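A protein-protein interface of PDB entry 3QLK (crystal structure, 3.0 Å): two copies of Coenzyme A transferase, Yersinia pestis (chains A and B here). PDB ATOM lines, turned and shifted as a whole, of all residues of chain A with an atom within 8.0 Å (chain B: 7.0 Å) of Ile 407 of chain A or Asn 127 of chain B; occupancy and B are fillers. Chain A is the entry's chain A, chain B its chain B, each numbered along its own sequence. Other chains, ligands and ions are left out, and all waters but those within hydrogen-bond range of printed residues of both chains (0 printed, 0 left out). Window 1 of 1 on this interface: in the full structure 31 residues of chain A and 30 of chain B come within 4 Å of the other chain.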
ATOM      1  N   THR A 344       8.591  28.782   3.961  1.00  0.00           N
ATOM      2  CA  THR A 344       7.183  28.565   3.606  1.00  0.00           C
ATOM      3  C   THR A 344       5.990  29.538   3.905  1.00  0.00           C
ATOM      4  O   THR A 344       4.905  29.297   3.378  1.00  0.00           O
ATOM      5  CB  THR A 344       6.770  27.244   4.260  1.00  0.00           C
ATOM      6  OG1 THR A 344       6.718  27.418   5.682  1.00  0.00           O
ATOM      7  CG2 THR A 344       7.849  26.239   4.000  1.00  0.00           C
ATOM      8  N   GLY A 345       6.080  30.565   4.740  1.00  0.00           N
ATOM      9  CA  GLY A 345       6.988  30.673   5.829  1.00  0.00           C
ATOM     10  C   GLY A 345       6.181  30.669   7.125  1.00  0.00           C
ATOM     11  O   GLY A 345       5.424  31.581   7.465  1.00  0.00           O
ATOM     12  N   ALA A 346       6.377  29.583   7.844  1.00  0.00           N
ATOM     13  CA  ALA A 346       5.879  29.351   9.171  1.00  0.00           C
ATOM     14  C   ALA A 346       6.762  30.225  10.060  1.00  0.00           C
ATOM     15  O   ALA A 346       7.861  30.584   9.662  1.00  0.00           O
ATOM     16  CB  ALA A 346       5.988  27.885   9.524  1.00  0.00           C
ATOM     17  N   LEU A 364      -1.476  33.519  17.978  1.00  0.00           N
ATOM     18  CA  LEU A 364      -2.231  32.935  16.877  1.00  0.00           C
ATOM     19  C   LEU A 364      -3.708  33.349  16.836  1.00  0.00           C
ATOM     20  O   LEU A 364      -4.252  33.520  15.755  1.00  0.00           O
ATOM     21  CB  LEU A 364      -2.104  31.424  16.920  1.00  0.00           C
ATOM     22  CG  LEU A 364      -2.734  30.746  15.710  1.00  0.00           C
ATOM     23  CD1 LEU A 364      -2.038  31.298  14.488  1.00  0.00           C
ATOM     24  CD2 LEU A 364      -2.578  29.251  15.759  1.00  0.00           C
ATOM     25  N   VAL A 367      -3.505  36.576  14.889  1.00  0.00           N
ATOM     26  CA  VAL A 367      -3.236  36.380  13.468  1.00  0.00           C
ATOM     27  C   VAL A 367      -4.533  36.036  12.732  1.00  0.00           C
ATOM     28  O   VAL A 367      -4.802  36.570  11.644  1.00  0.00           O
ATOM     29  CB  VAL A 367      -2.177  35.269  13.202  1.00  0.00           C
ATOM     30  CG1 VAL A 367      -2.170  34.838  11.748  1.00  0.00           C
ATOM     31  CG2 VAL A 367      -0.796  35.720  13.676  1.00  0.00           C
ATOM     32  N   ARG A 368      -5.304  35.100  13.284  1.00  0.00           N
ATOM     33  CA  ARG A 368      -6.560  34.738  12.658  1.00  0.00           C
ATOM     34  C   ARG A 368      -7.569  35.849  12.734  1.00  0.00           C
ATOM     35  O   ARG A 368      -8.215  36.188  11.738  1.00  0.00           O
ATOM     36  CB  ARG A 368      -7.168  33.472  13.252  1.00  0.00           C
ATOM     37  CG  ARG A 368      -6.261  32.290  12.885  1.00  0.00           C
ATOM     38  CD  ARG A 368      -6.453  30.954  13.562  1.00  0.00           C
ATOM     39  NE  ARG A 368      -6.814  31.011  14.964  1.00  0.00           N
ATOM     40  CZ  ARG A 368      -6.788  29.943  15.758  1.00  0.00           C
ATOM     41  NH1 ARG A 368      -6.408  28.755  15.242  1.00  0.00           N
ATOM     42  NH2 ARG A 368      -7.122  30.067  17.055  1.00  0.00           N
ATOM     43  N   TYR A 371      -6.794  38.886  10.350  1.00  0.00           N
ATOM     44  CA  TYR A 371      -7.043  38.600   8.941  1.00  0.00           C
ATOM     45  C   TYR A 371      -8.538  38.623   8.642  1.00  0.00           C
ATOM     46  O   TYR A 371      -8.959  39.096   7.570  1.00  0.00           O
ATOM     47  CB  TYR A 371      -6.413  37.268   8.522  1.00  0.00           C
ATOM     48  CG  TYR A 371      -6.536  37.013   7.036  1.00  0.00           C
ATOM     49  CD1 TYR A 371      -5.858  37.805   6.113  1.00  0.00           C
ATOM     50  CD2 TYR A 371      -7.325  35.964   6.552  1.00  0.00           C
ATOM     51  CE1 TYR A 371      -5.985  37.572   4.743  1.00  0.00           C
ATOM     52  CE2 TYR A 371      -7.448  35.713   5.177  1.00  0.00           C
ATOM     53  CZ  TYR A 371      -6.780  36.523   4.285  1.00  0.00           C
ATOM     54  OH  TYR A 371      -6.896  36.308   2.931  1.00  0.00           O
ATOM     55  N   VAL A 402       5.496  24.683  15.122  1.00  0.00           N
ATOM     56  CA  VAL A 402       5.736  26.047  14.752  1.00  0.00           C
ATOM     57  C   VAL A 402       4.872  26.952  15.656  1.00  0.00           C
ATOM     58  O   VAL A 402       3.974  26.464  16.334  1.00  0.00           O
ATOM     59  CB  VAL A 402       5.416  26.181  13.260  1.00  0.00           C
ATOM     60  CG1 VAL A 402       3.912  26.276  13.055  1.00  0.00           C
ATOM     61  CG2 VAL A 402       6.115  27.361  12.676  1.00  0.00           C
ATOM     62  N   THR A 404       3.346  30.143  14.350  1.00  0.00           N
ATOM     63  CA  THR A 404       2.363  30.525  13.376  1.00  0.00           C
ATOM     64  C   THR A 404       2.461  29.595  12.201  1.00  0.00           C
ATOM     65  O   THR A 404       3.481  29.555  11.542  1.00  0.00           O
ATOM     66  CB  THR A 404       2.655  31.968  12.940  1.00  0.00           C
ATOM     67  OG1 THR A 404       2.659  32.833  14.088  1.00  0.00           O
ATOM     68  CG2 THR A 404       1.663  32.444  11.925  1.00  0.00           C
ATOM     69  N   PRO A 405       1.400  28.828  11.933  1.00  0.00           N
ATOM     70  CA  PRO A 405       1.422  27.880  10.814  1.00  0.00           C
ATOM     71  C   PRO A 405       1.524  28.655   9.497  1.00  0.00           C
ATOM     72  O   PRO A 405       1.003  29.773   9.406  1.00  0.00           O
ATOM     73  CB  PRO A 405       0.060  27.195  10.920  1.00  0.00           C
ATOM     74  CG  PRO A 405      -0.337  27.386  12.357  1.00  0.00           C
ATOM     75  CD  PRO A 405       0.156  28.740  12.707  1.00  0.00           C
ATOM     76  N   ARG A 406       2.123  28.068   8.466  1.00  0.00           N
ATOM     77  CA  ARG A 406       2.233  28.807   7.220  1.00  0.00           C
ATOM     78  C   ARG A 406       0.894  29.172   6.584  1.00  0.00           C
ATOM     79  O   ARG A 406       0.817  30.151   5.851  1.00  0.00           O
ATOM     80  CB  ARG A 406       3.050  28.006   6.210  1.00  0.00           C
ATOM     81  CG  ARG A 406       2.304  26.771   5.675  1.00  0.00           C
ATOM     82  CD  ARG A 406       2.984  26.147   4.461  1.00  0.00           C
ATOM     83  NE  ARG A 406       3.865  25.014   4.743  1.00  0.00           N
ATOM     84  CZ  ARG A 406       3.560  23.743   4.467  1.00  0.00           C
ATOM     85  NH1 ARG A 406       2.375  23.427   3.932  1.00  0.00           N
ATOM     86  NH2 ARG A 406       4.437  22.781   4.748  1.00  0.00           N
ATOM     87  N   ILE A 407      -0.177  28.447   6.899  1.00  0.00           N
ATOM     88  CA  ILE A 407      -1.485  28.748   6.296  1.00  0.00           C
ATOM     89  C   ILE A 407      -2.137  29.962   6.919  1.00  0.00           C
ATOM     90  O   ILE A 407      -3.086  30.509   6.381  1.00  0.00           O
ATOM     91  CB  ILE A 407      -2.482  27.571   6.338  1.00  0.00           C
ATOM     92  CG1 ILE A 407      -2.668  27.046   7.755  1.00  0.00           C
ATOM     93  CG2 ILE A 407      -2.009  26.460   5.477  1.00  0.00           C
ATOM     94  CD1 ILE A 407      -3.645  25.888   7.829  1.00  0.00           C
ATOM     95  N   ASP A 408      -1.607  30.387   8.051  1.00  0.00           N
ATOM     96  CA  ASP A 408      -2.165  31.514   8.771  1.00  0.00           C
ATOM     97  C   ASP A 408      -1.365  32.791   8.652  1.00  0.00           C
ATOM     98  O   ASP A 408      -1.920  33.857   8.840  1.00  0.00           O
ATOM     99  CB  ASP A 408      -2.357  31.164  10.257  1.00  0.00           C
ATOM    100  CG  ASP A 408      -3.469  30.120  10.483  1.00  0.00           C
ATOM    101  OD1 ASP A 408      -4.613  30.330   9.974  1.00  0.00           O
ATOM    102  OD2 ASP A 408      -3.209  29.089  11.150  1.00  0.00           O
ATOM    103  N   THR A 409      -0.107  32.714   8.246  1.00  0.00           N
ATOM    104  CA  THR A 409       0.719  33.912   8.172  1.00  0.00           C
ATOM    105  C   THR A 409       0.105  34.894   7.202  1.00  0.00           C
ATOM    106  O   THR A 409      -0.389  34.492   6.150  1.00  0.00           O
ATOM    107  CB  THR A 409       2.148  33.554   7.753  1.00  0.00           C
ATOM    108  OG1 THR A 409       2.601  32.428   8.501  1.00  0.00           O
ATOM    109  CG2 THR A 409       3.092  34.734   7.889  1.00  0.00           C
ATOM    110  N   HIS A 410       0.097  36.174   7.557  1.00  0.00           N
ATOM    111  CA  HIS A 410      -0.491  37.161   6.658  1.00  0.00           C
ATOM    112  C   HIS A 410       0.625  38.032   6.075  1.00  0.00           C
ATOM    113  O   HIS A 410       1.040  37.856   4.933  1.00  0.00           O
ATOM    114  CB  HIS A 410      -1.504  38.024   7.410  1.00  0.00           C
ATOM    115  CG  HIS A 410      -2.312  38.921   6.524  1.00  0.00           C
ATOM    116  ND1 HIS A 410      -3.076  39.960   7.015  1.00  0.00           N
ATOM    117  CD2 HIS A 410      -2.452  38.952   5.177  1.00  0.00           C
ATOM    118  CE1 HIS A 410      -3.671  40.579   6.011  1.00  0.00           C
ATOM    119  NE2 HIS A 410      -3.315  39.984   4.884  1.00  0.00           N
ATOM    120  N   LEU A 421       1.726  37.001   2.384  1.00  0.00           N
ATOM    121  CA  LEU A 421       1.857  35.617   1.918  1.00  0.00           C
ATOM    122  C   LEU A 421       0.517  34.956   1.484  1.00  0.00           C
ATOM    123  O   LEU A 421       0.538  33.860   0.925  1.00  0.00           O
ATOM    124  CB  LEU A 421       2.546  34.697   2.922  1.00  0.00           C
ATOM    125  CG  LEU A 421       3.936  35.160   3.298  1.00  0.00           C
ATOM    126  CD1 LEU A 421       4.454  34.177   4.335  1.00  0.00           C
ATOM    127  CD2 LEU A 421       4.849  35.136   2.117  1.00  0.00           C
ATOM    128  N   LYS A 422      -0.633  35.547   1.809  1.00  0.00           N
ATOM    129  CA  LYS A 422      -1.897  34.878   1.532  1.00  0.00           C
ATOM    130  C   LYS A 422      -2.097  34.657   0.026  1.00  0.00           C
ATOM    131  O   LYS A 422      -2.082  35.626  -0.752  1.00  0.00           O
ATOM    132  CB  LYS A 422      -3.075  35.653   2.122  1.00  0.00           C
ATOM    133  CG  LYS A 422      -3.202  35.713   3.633  1.00  0.00           C
ATOM    134  CD  LYS A 422      -3.697  34.399   4.186  1.00  0.00           C
ATOM    135  CE  LYS A 422      -4.020  34.478   5.658  1.00  0.00           C
ATOM    136  NZ  LYS A 422      -4.439  33.170   6.252  1.00  0.00           N
ATOM    137  N   GLY A 423      -2.356  33.402  -0.367  1.00  0.00           N
ATOM    138  CA  GLY A 423      -2.626  33.089  -1.756  1.00  0.00           C
ATOM    139  C   GLY A 423      -1.406  32.803  -2.617  1.00  0.00           C
ATOM    140  O   GLY A 423      -1.513  32.426  -3.807  1.00  0.00           O
ATOM    141  N   ARG A 429       6.137  32.058  -2.249  1.00  0.00           N
ATOM    142  CA  ARG A 429       6.467  32.322  -0.846  1.00  0.00           C
ATOM    143  C   ARG A 429       8.005  32.278  -0.623  1.00  0.00           C
ATOM    144  O   ARG A 429       8.599  33.241  -0.130  1.00  0.00           O
ATOM    145  CB  ARG A 429       5.757  31.284   0.037  1.00  0.00           C
ATOM    146  CG  ARG A 429       4.209  31.455   0.097  1.00  0.00           C
ATOM    147  CD  ARG A 429       3.517  30.405   1.017  1.00  0.00           C
ATOM    148  NE  ARG A 429       2.853  30.945   2.206  1.00  0.00           N
ATOM    149  CZ  ARG A 429       1.538  30.987   2.356  1.00  0.00           C
ATOM    150  NH1 ARG A 429       0.746  30.540   1.384  1.00  0.00           N
ATOM    151  NH2 ARG A 429       1.002  31.478   3.461  1.00  0.00           N
ATOM    152  N   PHE B  75      -9.243  22.617  -5.344  1.00  0.00           N
ATOM    153  CA  PHE B  75      -9.217  21.676  -4.215  1.00  0.00           C
ATOM    154  C   PHE B  75      -9.863  20.379  -4.640  1.00  0.00           C
ATOM    155  O   PHE B  75     -10.786  20.385  -5.473  1.00  0.00           O
ATOM    156  CB  PHE B  75     -10.074  22.143  -3.027  1.00  0.00           C
ATOM    157  CG  PHE B  75      -9.505  23.170  -2.123  1.00  0.00           C
ATOM    158  CD1 PHE B  75      -8.874  22.751  -0.952  1.00  0.00           C
ATOM    159  CD2 PHE B  75      -9.580  24.527  -2.403  1.00  0.00           C
ATOM    160  CE1 PHE B  75      -8.384  23.666  -0.039  1.00  0.00           C
ATOM    161  CE2 PHE B  75      -9.057  25.469  -1.499  1.00  0.00           C
ATOM    162  CZ  PHE B  75      -8.452  25.031  -0.325  1.00  0.00           C
ATOM    163  N   MET B  99      -4.491  23.287  -3.868  1.00  0.00           N
ATOM    164  CA  MET B  99      -4.584  23.841  -2.516  1.00  0.00           C
ATOM    165  C   MET B  99      -4.711  22.755  -1.442  1.00  0.00           C
ATOM    166  O   MET B  99      -4.477  23.010  -0.257  1.00  0.00           O
ATOM    167  CB  MET B  99      -5.687  24.897  -2.471  1.00  0.00           C
ATOM    168  CG  MET B  99      -5.428  26.034  -3.427  1.00  0.00           C
ATOM    169  SD  MET B  99      -6.805  27.190  -3.540  1.00  0.00           S
ATOM    170  CE  MET B  99      -6.596  28.134  -2.033  1.00  0.00           C
ATOM    171  N   TYR B 123       2.034  24.069  -4.954  1.00  0.00           N
ATOM    172  CA  TYR B 123       1.112  23.962  -3.840  1.00  0.00           C
ATOM    173  C   TYR B 123       0.850  25.361  -3.283  1.00  0.00           C
ATOM    174  O   TYR B 123       1.785  26.152  -3.096  1.00  0.00           O
ATOM    175  CB  TYR B 123       1.677  23.031  -2.770  1.00  0.00           C
ATOM    176  CG  TYR B 123       0.848  22.928  -1.505  1.00  0.00           C
ATOM    177  CD1 TYR B 123      -0.424  22.335  -1.525  1.00  0.00           C
ATOM    178  CD2 TYR B 123       1.352  23.364  -0.273  1.00  0.00           C
ATOM    179  CE1 TYR B 123      -1.195  22.221  -0.349  1.00  0.00           C
ATOM    180  CE2 TYR B 123       0.596  23.253   0.903  1.00  0.00           C
ATOM    181  CZ  TYR B 123      -0.676  22.685   0.865  1.00  0.00           C
ATOM    182  OH  TYR B 123      -1.419  22.579   2.034  1.00  0.00           O
ATOM    183  N   VAL B 124      -0.431  25.666  -3.045  1.00  0.00           N
ATOM    184  CA  VAL B 124      -0.804  26.935  -2.440  1.00  0.00           C
ATOM    185  C   VAL B 124      -1.364  26.687  -1.049  1.00  0.00           C
ATOM    186  O   VAL B 124      -2.541  26.325  -0.901  1.00  0.00           O
ATOM    187  CB  VAL B 124      -1.908  27.626  -3.282  1.00  0.00           C
ATOM    188  CG1 VAL B 124      -2.373  28.946  -2.616  1.00  0.00           C
ATOM    189  CG2 VAL B 124      -1.443  27.861  -4.707  1.00  0.00           C
ATOM    190  N   PRO B 125      -0.577  26.979  -0.011  1.00  0.00           N
ATOM    191  CA  PRO B 125      -1.073  26.765   1.351  1.00  0.00           C
ATOM    192  C   PRO B 125      -2.286  27.641   1.645  1.00  0.00           C
ATOM    193  O   PRO B 125      -2.246  28.847   1.382  1.00  0.00           O
ATOM    194  CB  PRO B 125       0.105  27.193   2.224  1.00  0.00           C
ATOM    195  CG  PRO B 125       1.289  27.074   1.344  1.00  0.00           C
ATOM    196  CD  PRO B 125       0.813  27.440  -0.022  1.00  0.00           C
ATOM    197  N   SER B 126      -3.301  27.051   2.273  1.00  0.00           N
ATOM    198  CA  SER B 126      -4.502  27.789   2.588  1.00  0.00           C
ATOM    199  C   SER B 126      -5.449  27.065   3.554  1.00  0.00           C
ATOM    200  O   SER B 126      -5.384  25.845   3.700  1.00  0.00           O
ATOM    201  CB  SER B 126      -5.227  28.019   1.284  1.00  0.00           C
ATOM    202  OG  SER B 126      -5.887  26.830   0.934  1.00  0.00           O
ATOM    203  N   ASN B 127      -6.454  27.803   4.034  1.00  0.00           N
ATOM    204  CA  ASN B 127      -7.580  27.241   4.788  1.00  0.00           C
ATOM    205  C   ASN B 127      -8.757  27.012   3.888  1.00  0.00           C
ATOM    206  O   ASN B 127      -9.202  27.926   3.201  1.00  0.00           O
ATOM    207  CB  ASN B 127      -7.998  28.236   5.874  1.00  0.00           C
ATOM    208  CG  ASN B 127      -7.011  28.316   7.017  1.00  0.00           C
ATOM    209  OD1 ASN B 127      -6.820  27.353   7.759  1.00  0.00           O
ATOM    210  ND2 ASN B 127      -6.352  29.476   7.152  1.00  0.00           N
ATOM    211  N   PHE B 128      -9.277  25.794   3.877  1.00  0.00           N
ATOM    212  CA  PHE B 128     -10.423  25.541   3.034  1.00  0.00           C
ATOM    213  C   PHE B 128     -11.512  26.597   3.209  1.00  0.00           C
ATOM    214  O   PHE B 128     -12.086  27.078   2.238  1.00  0.00           O
ATOM    215  CB  PHE B 128     -10.952  24.137   3.273  1.00  0.00           C
ATOM    216  CG  PHE B 128     -12.077  23.770   2.386  1.00  0.00           C
ATOM    217  CD1 PHE B 128     -12.049  24.165   1.064  1.00  0.00           C
ATOM    218  CD2 PHE B 128     -13.051  22.886   2.796  1.00  0.00           C
ATOM    219  CE1 PHE B 128     -13.031  23.804   0.205  1.00  0.00           C
ATOM    220  CE2 PHE B 128     -14.047  22.502   1.932  1.00  0.00           C
ATOM    221  CZ  PHE B 128     -14.035  22.964   0.631  1.00  0.00           C
ATOM    222  N   HIS B 129     -11.780  26.978   4.449  1.00  0.00           N
ATOM    223  CA  HIS B 129     -12.830  27.954   4.687  1.00  0.00           C
ATOM    224  C   HIS B 129     -12.493  29.446   4.291  1.00  0.00           C
ATOM    225  O   HIS B 129     -13.295  30.369   4.331  1.00  0.00           O
ATOM    226  CB  HIS B 129     -13.170  27.933   6.169  1.00  0.00           C
ATOM    227  CG  HIS B 129     -12.016  28.258   7.062  1.00  0.00           C
ATOM    228  ND1 HIS B 129     -10.993  27.357   7.310  1.00  0.00           N
ATOM    229  CD2 HIS B 129     -11.710  29.383   7.758  1.00  0.00           C
ATOM    230  CE1 HIS B 129     -10.107  27.909   8.121  1.00  0.00           C
ATOM    231  NE2 HIS B 129     -10.519  29.138   8.411  1.00  0.00           N
ATOM    232  N   GLN B 130     -11.279  29.627   3.796  1.00  0.00           N
ATOM    233  CA  GLN B 130     -10.838  30.957   3.359  1.00  0.00           C
ATOM    234  C   GLN B 130     -10.768  30.837   1.831  1.00  0.00           C
ATOM    235  O   GLN B 130     -10.364  31.785   1.141  1.00  0.00           O
ATOM    236  CB  GLN B 130      -9.520  31.500   3.891  1.00  0.00           C
ATOM    237  CG  GLN B 130      -9.549  31.768   5.348  1.00  0.00           C
ATOM    238  CD  GLN B 130      -8.181  32.094   5.942  1.00  0.00           C
ATOM    239  OE1 GLN B 130      -7.124  31.778   5.368  1.00  0.00           O
ATOM    240  NE2 GLN B 130      -8.199  32.667   7.135  1.00  0.00           N
ATOM    241  N   ALA B 131     -11.054  29.641   1.312  1.00  0.00           N
ATOM    242  CA  ALA B 131     -10.894  29.435  -0.111  1.00  0.00           C
ATOM    243  C   ALA B 131     -11.649  30.459  -0.930  1.00  0.00           C
ATOM    244  O   ALA B 131     -11.099  31.021  -1.850  1.00  0.00           O
ATOM    245  CB  ALA B 131     -11.261  28.035  -0.509  1.00  0.00           C
ATOM    246  N   PRO B 132     -12.877  30.790  -0.537  1.00  0.00           N
ATOM    247  CA  PRO B 132     -13.594  31.759  -1.370  1.00  0.00           C
ATOM    248  C   PRO B 132     -12.861  33.105  -1.422  1.00  0.00           C
ATOM    249  O   PRO B 132     -12.771  33.680  -2.496  1.00  0.00           O
ATOM    250  CB  PRO B 132     -14.949  31.889  -0.668  1.00  0.00           C
ATOM    251  CG  PRO B 132     -15.118  30.577   0.037  1.00  0.00           C
ATOM    252  CD  PRO B 132     -13.731  30.275   0.547  1.00  0.00           C
ATOM    253  N   LEU B 134      -9.524  33.747  -0.633  1.00  0.00           N
ATOM    254  CA  LEU B 134      -8.182  33.581  -1.190  1.00  0.00           C
ATOM    255  C   LEU B 134      -8.273  33.596  -2.698  1.00  0.00           C
ATOM    256  O   LEU B 134      -7.513  34.277  -3.369  1.00  0.00           O
ATOM    257  CB  LEU B 134      -7.504  32.295  -0.728  1.00  0.00           C
ATOM    258  CG  LEU B 134      -6.820  32.275   0.630  1.00  0.00           C
ATOM    259  CD1 LEU B 134      -6.680  30.844   1.077  1.00  0.00           C
ATOM    260  CD2 LEU B 134      -5.473  32.933   0.552  1.00  0.00           C
ATOM    261  N   VAL B 317     -18.488  27.382   1.873  1.00  0.00           N
ATOM    262  CA  VAL B 317     -17.556  26.848   2.852  1.00  0.00           C
ATOM    263  C   VAL B 317     -17.138  27.885   3.888  1.00  0.00           C
ATOM    264  O   VAL B 317     -16.771  27.523   5.004  1.00  0.00           O
ATOM    265  CB  VAL B 317     -16.330  26.189   2.200  1.00  0.00           C
ATOM    266  CG1 VAL B 317     -15.501  27.219   1.449  1.00  0.00           C
ATOM    267  CG2 VAL B 317     -15.495  25.461   3.257  1.00  0.00           C
ATOM    268  N   GLY B 362      -8.413  22.013   6.572  1.00  0.00           N
ATOM    269  CA  GLY B 362      -9.565  21.278   6.058  1.00  0.00           C
ATOM    270  C   GLY B 362     -10.591  20.783   7.093  1.00  0.00           C
ATOM    271  O   GLY B 362     -11.768  21.181   7.086  1.00  0.00           O
ATOM    272  N   LEU B 364      -9.675  20.942  10.422  1.00  0.00           N
ATOM    273  CA  LEU B 364      -9.277  21.589  11.692  1.00  0.00           C
ATOM    274  C   LEU B 364     -10.378  22.539  12.198  1.00  0.00           C
ATOM    275  O   LEU B 364     -10.584  22.720  13.392  1.00  0.00           O
ATOM    276  CB  LEU B 364      -7.933  22.306  11.583  1.00  0.00           C
ATOM    277  CG  LEU B 364      -7.430  22.936  12.893  1.00  0.00           C
ATOM    278  CD1 LEU B 364      -7.451  21.938  14.035  1.00  0.00           C
ATOM    279  CD2 LEU B 364      -6.050  23.527  12.744  1.00  0.00           C
ATOM    280  N   ASP B 365     -11.089  23.115  11.244  1.00  0.00           N
ATOM    281  CA  ASP B 365     -12.220  23.984  11.476  1.00  0.00           C
ATOM    282  C   ASP B 365     -13.274  23.293  12.376  1.00  0.00           C
ATOM    283  O   ASP B 365     -13.833  23.916  13.267  1.00  0.00           O
ATOM    284  CB  ASP B 365     -12.820  24.284  10.111  1.00  0.00           C
ATOM    285  CG  ASP B 365     -11.849  25.010   9.212  1.00  0.00           C
ATOM    286  OD1 ASP B 365     -11.042  25.810   9.769  1.00  0.00           O
ATOM    287  OD2 ASP B 365     -11.855  24.746   7.978  1.00  0.00           O
ATOM    288  N   ARG B 368     -12.008  22.586  15.934  1.00  0.00           N
ATOM    289  CA  ARG B 368     -12.214  23.802  16.685  1.00  0.00           C
ATOM    290  C   ARG B 368     -13.710  24.027  16.947  1.00  0.00           C
ATOM    291  O   ARG B 368     -14.117  24.209  18.086  1.00  0.00           O
ATOM    292  CB  ARG B 368     -11.593  24.975  15.927  1.00  0.00           C
ATOM    293  CG  ARG B 368     -10.033  24.861  15.930  1.00  0.00           C
ATOM    294  CD  ARG B 368      -9.351  25.804  14.965  1.00  0.00           C
ATOM    295  NE  ARG B 368      -9.694  27.194  15.224  1.00  0.00           N
ATOM    296  CZ  ARG B 368      -9.579  28.159  14.315  1.00  0.00           C
ATOM    297  NH1 ARG B 368      -9.182  27.814  13.084  1.00  0.00           N
ATOM    298  NH2 ARG B 368      -9.910  29.438  14.607  1.00  0.00           N
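O of Thr 344 of chain A is in hydrogen-bond range of NE of Arg 429 of chain A.
The backbone carbonyl oxygen (O) of Leu 421 of chain A lies within hydrogen-bond range of the guanidinium group (NH1) of Arg 429 of chain A (3.4 Å).
O of Arg 406 of chain A sits at hydrogen-bond distance from NH2 of Arg 429 of chain A (2.7 Å).
O of Ile 407 of chain A lies within hydrogen-bond range of NZ of Lys 422 of chain A, at 3.0 Å.
The side-chain amide oxygen (OE1) of Gln 130 of chain B sits at hydrogen-bond distance from the side-chain amide nitrogen (ND2) of Asn 127 of chain B (3.0 Å).
Of chain B, only Pro 125 (3.9 Å), Ser 126 (3.5 Å) and Asn 127 (3.5 Å) come within 4 Å of Ile 407 of chain A.
Of the printed residues of chain A, Val 124 of chain B touches Gly 423.
Ser 126 of chain B touches one residue of chain A.
Asn 127 of chain B touches just these residues of chain A: Ile 407 (3.5 Å) and Asp 408 (3.4 Å).
Of the printed residues of chain A, Leu 134 of chain B touches Lys 422 (3.8 Å) and Gly 423 (3.3 Å).
The nearest residue of chain B that does not touch Ile 407 of chain A is Gln 130 of chain B (4.4 Å).
The nearest printed residue of chain B that does not touch Arg 368 of chain A is Gln 130 of chain B (5.8 Å).
CD2 of Tyr 371 of chain A touches NE2 of Gln 130 of chain B (3.5 Å).
Tyr 123 of chain B touches Arg 406 of chain A (CE2 to NH1, 3.5 Å).
Pro 125 of chain B touches Arg 406 of chain A.
CB of Pro 125 of chain B touches CG2 of Ile 407 of chain A (3.9 Å).
Ser 126 of chain B touches Ile 407 of chain A (N to CG2, 3.5 Å).
OD1 of Asn 127 of chain B touches CD1 of Ile 407 of chain A, 3.5 Å away.
CD2 of Leu 134 of chain B touches C of Lys 422 of chain A, 3.8 Å away.
CG1 of Val 124 of chain B touches O of Gly 423 of chain A, 3.8 Å away.
CD2 of Leu 134 of chain B touches N of Gly 423 of chain A, 3.3 Å away.
The guanidinium group of Arg 368 of chain B sits close to the guanidinium group of Arg 368 of chain A (3.5 Å).
OE1 of Gln 130 of chain B lies within hydrogen-bond range of NZ of Lys 422 of chain A (3.2 Å).
The guanidinium group of Arg 429 of chain A lies close to the backbone carbonyl oxygen of Pro 125 of chain B.
The side-chain carboxylate (OD1) of Asp 408 of chain A is in hydrogen-bond range of the side-chain amide nitrogen (ND2) of Asn 127 of chain B.
Arg 368 of chain B touches its own counterpart, Arg 368 of chain A.
2 positions are printed for both chains.
Printed residues of chain A that touch a printed residue of chain B: Arg 368, Tyr 371, Arg 406, Ile 407, Asp 408, Lys 422, Gly 423 and Arg 429.
Hydrophobic or aromatic side chains of chain A that line the printed part of chain B: Tyr 371 and Ile 407.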
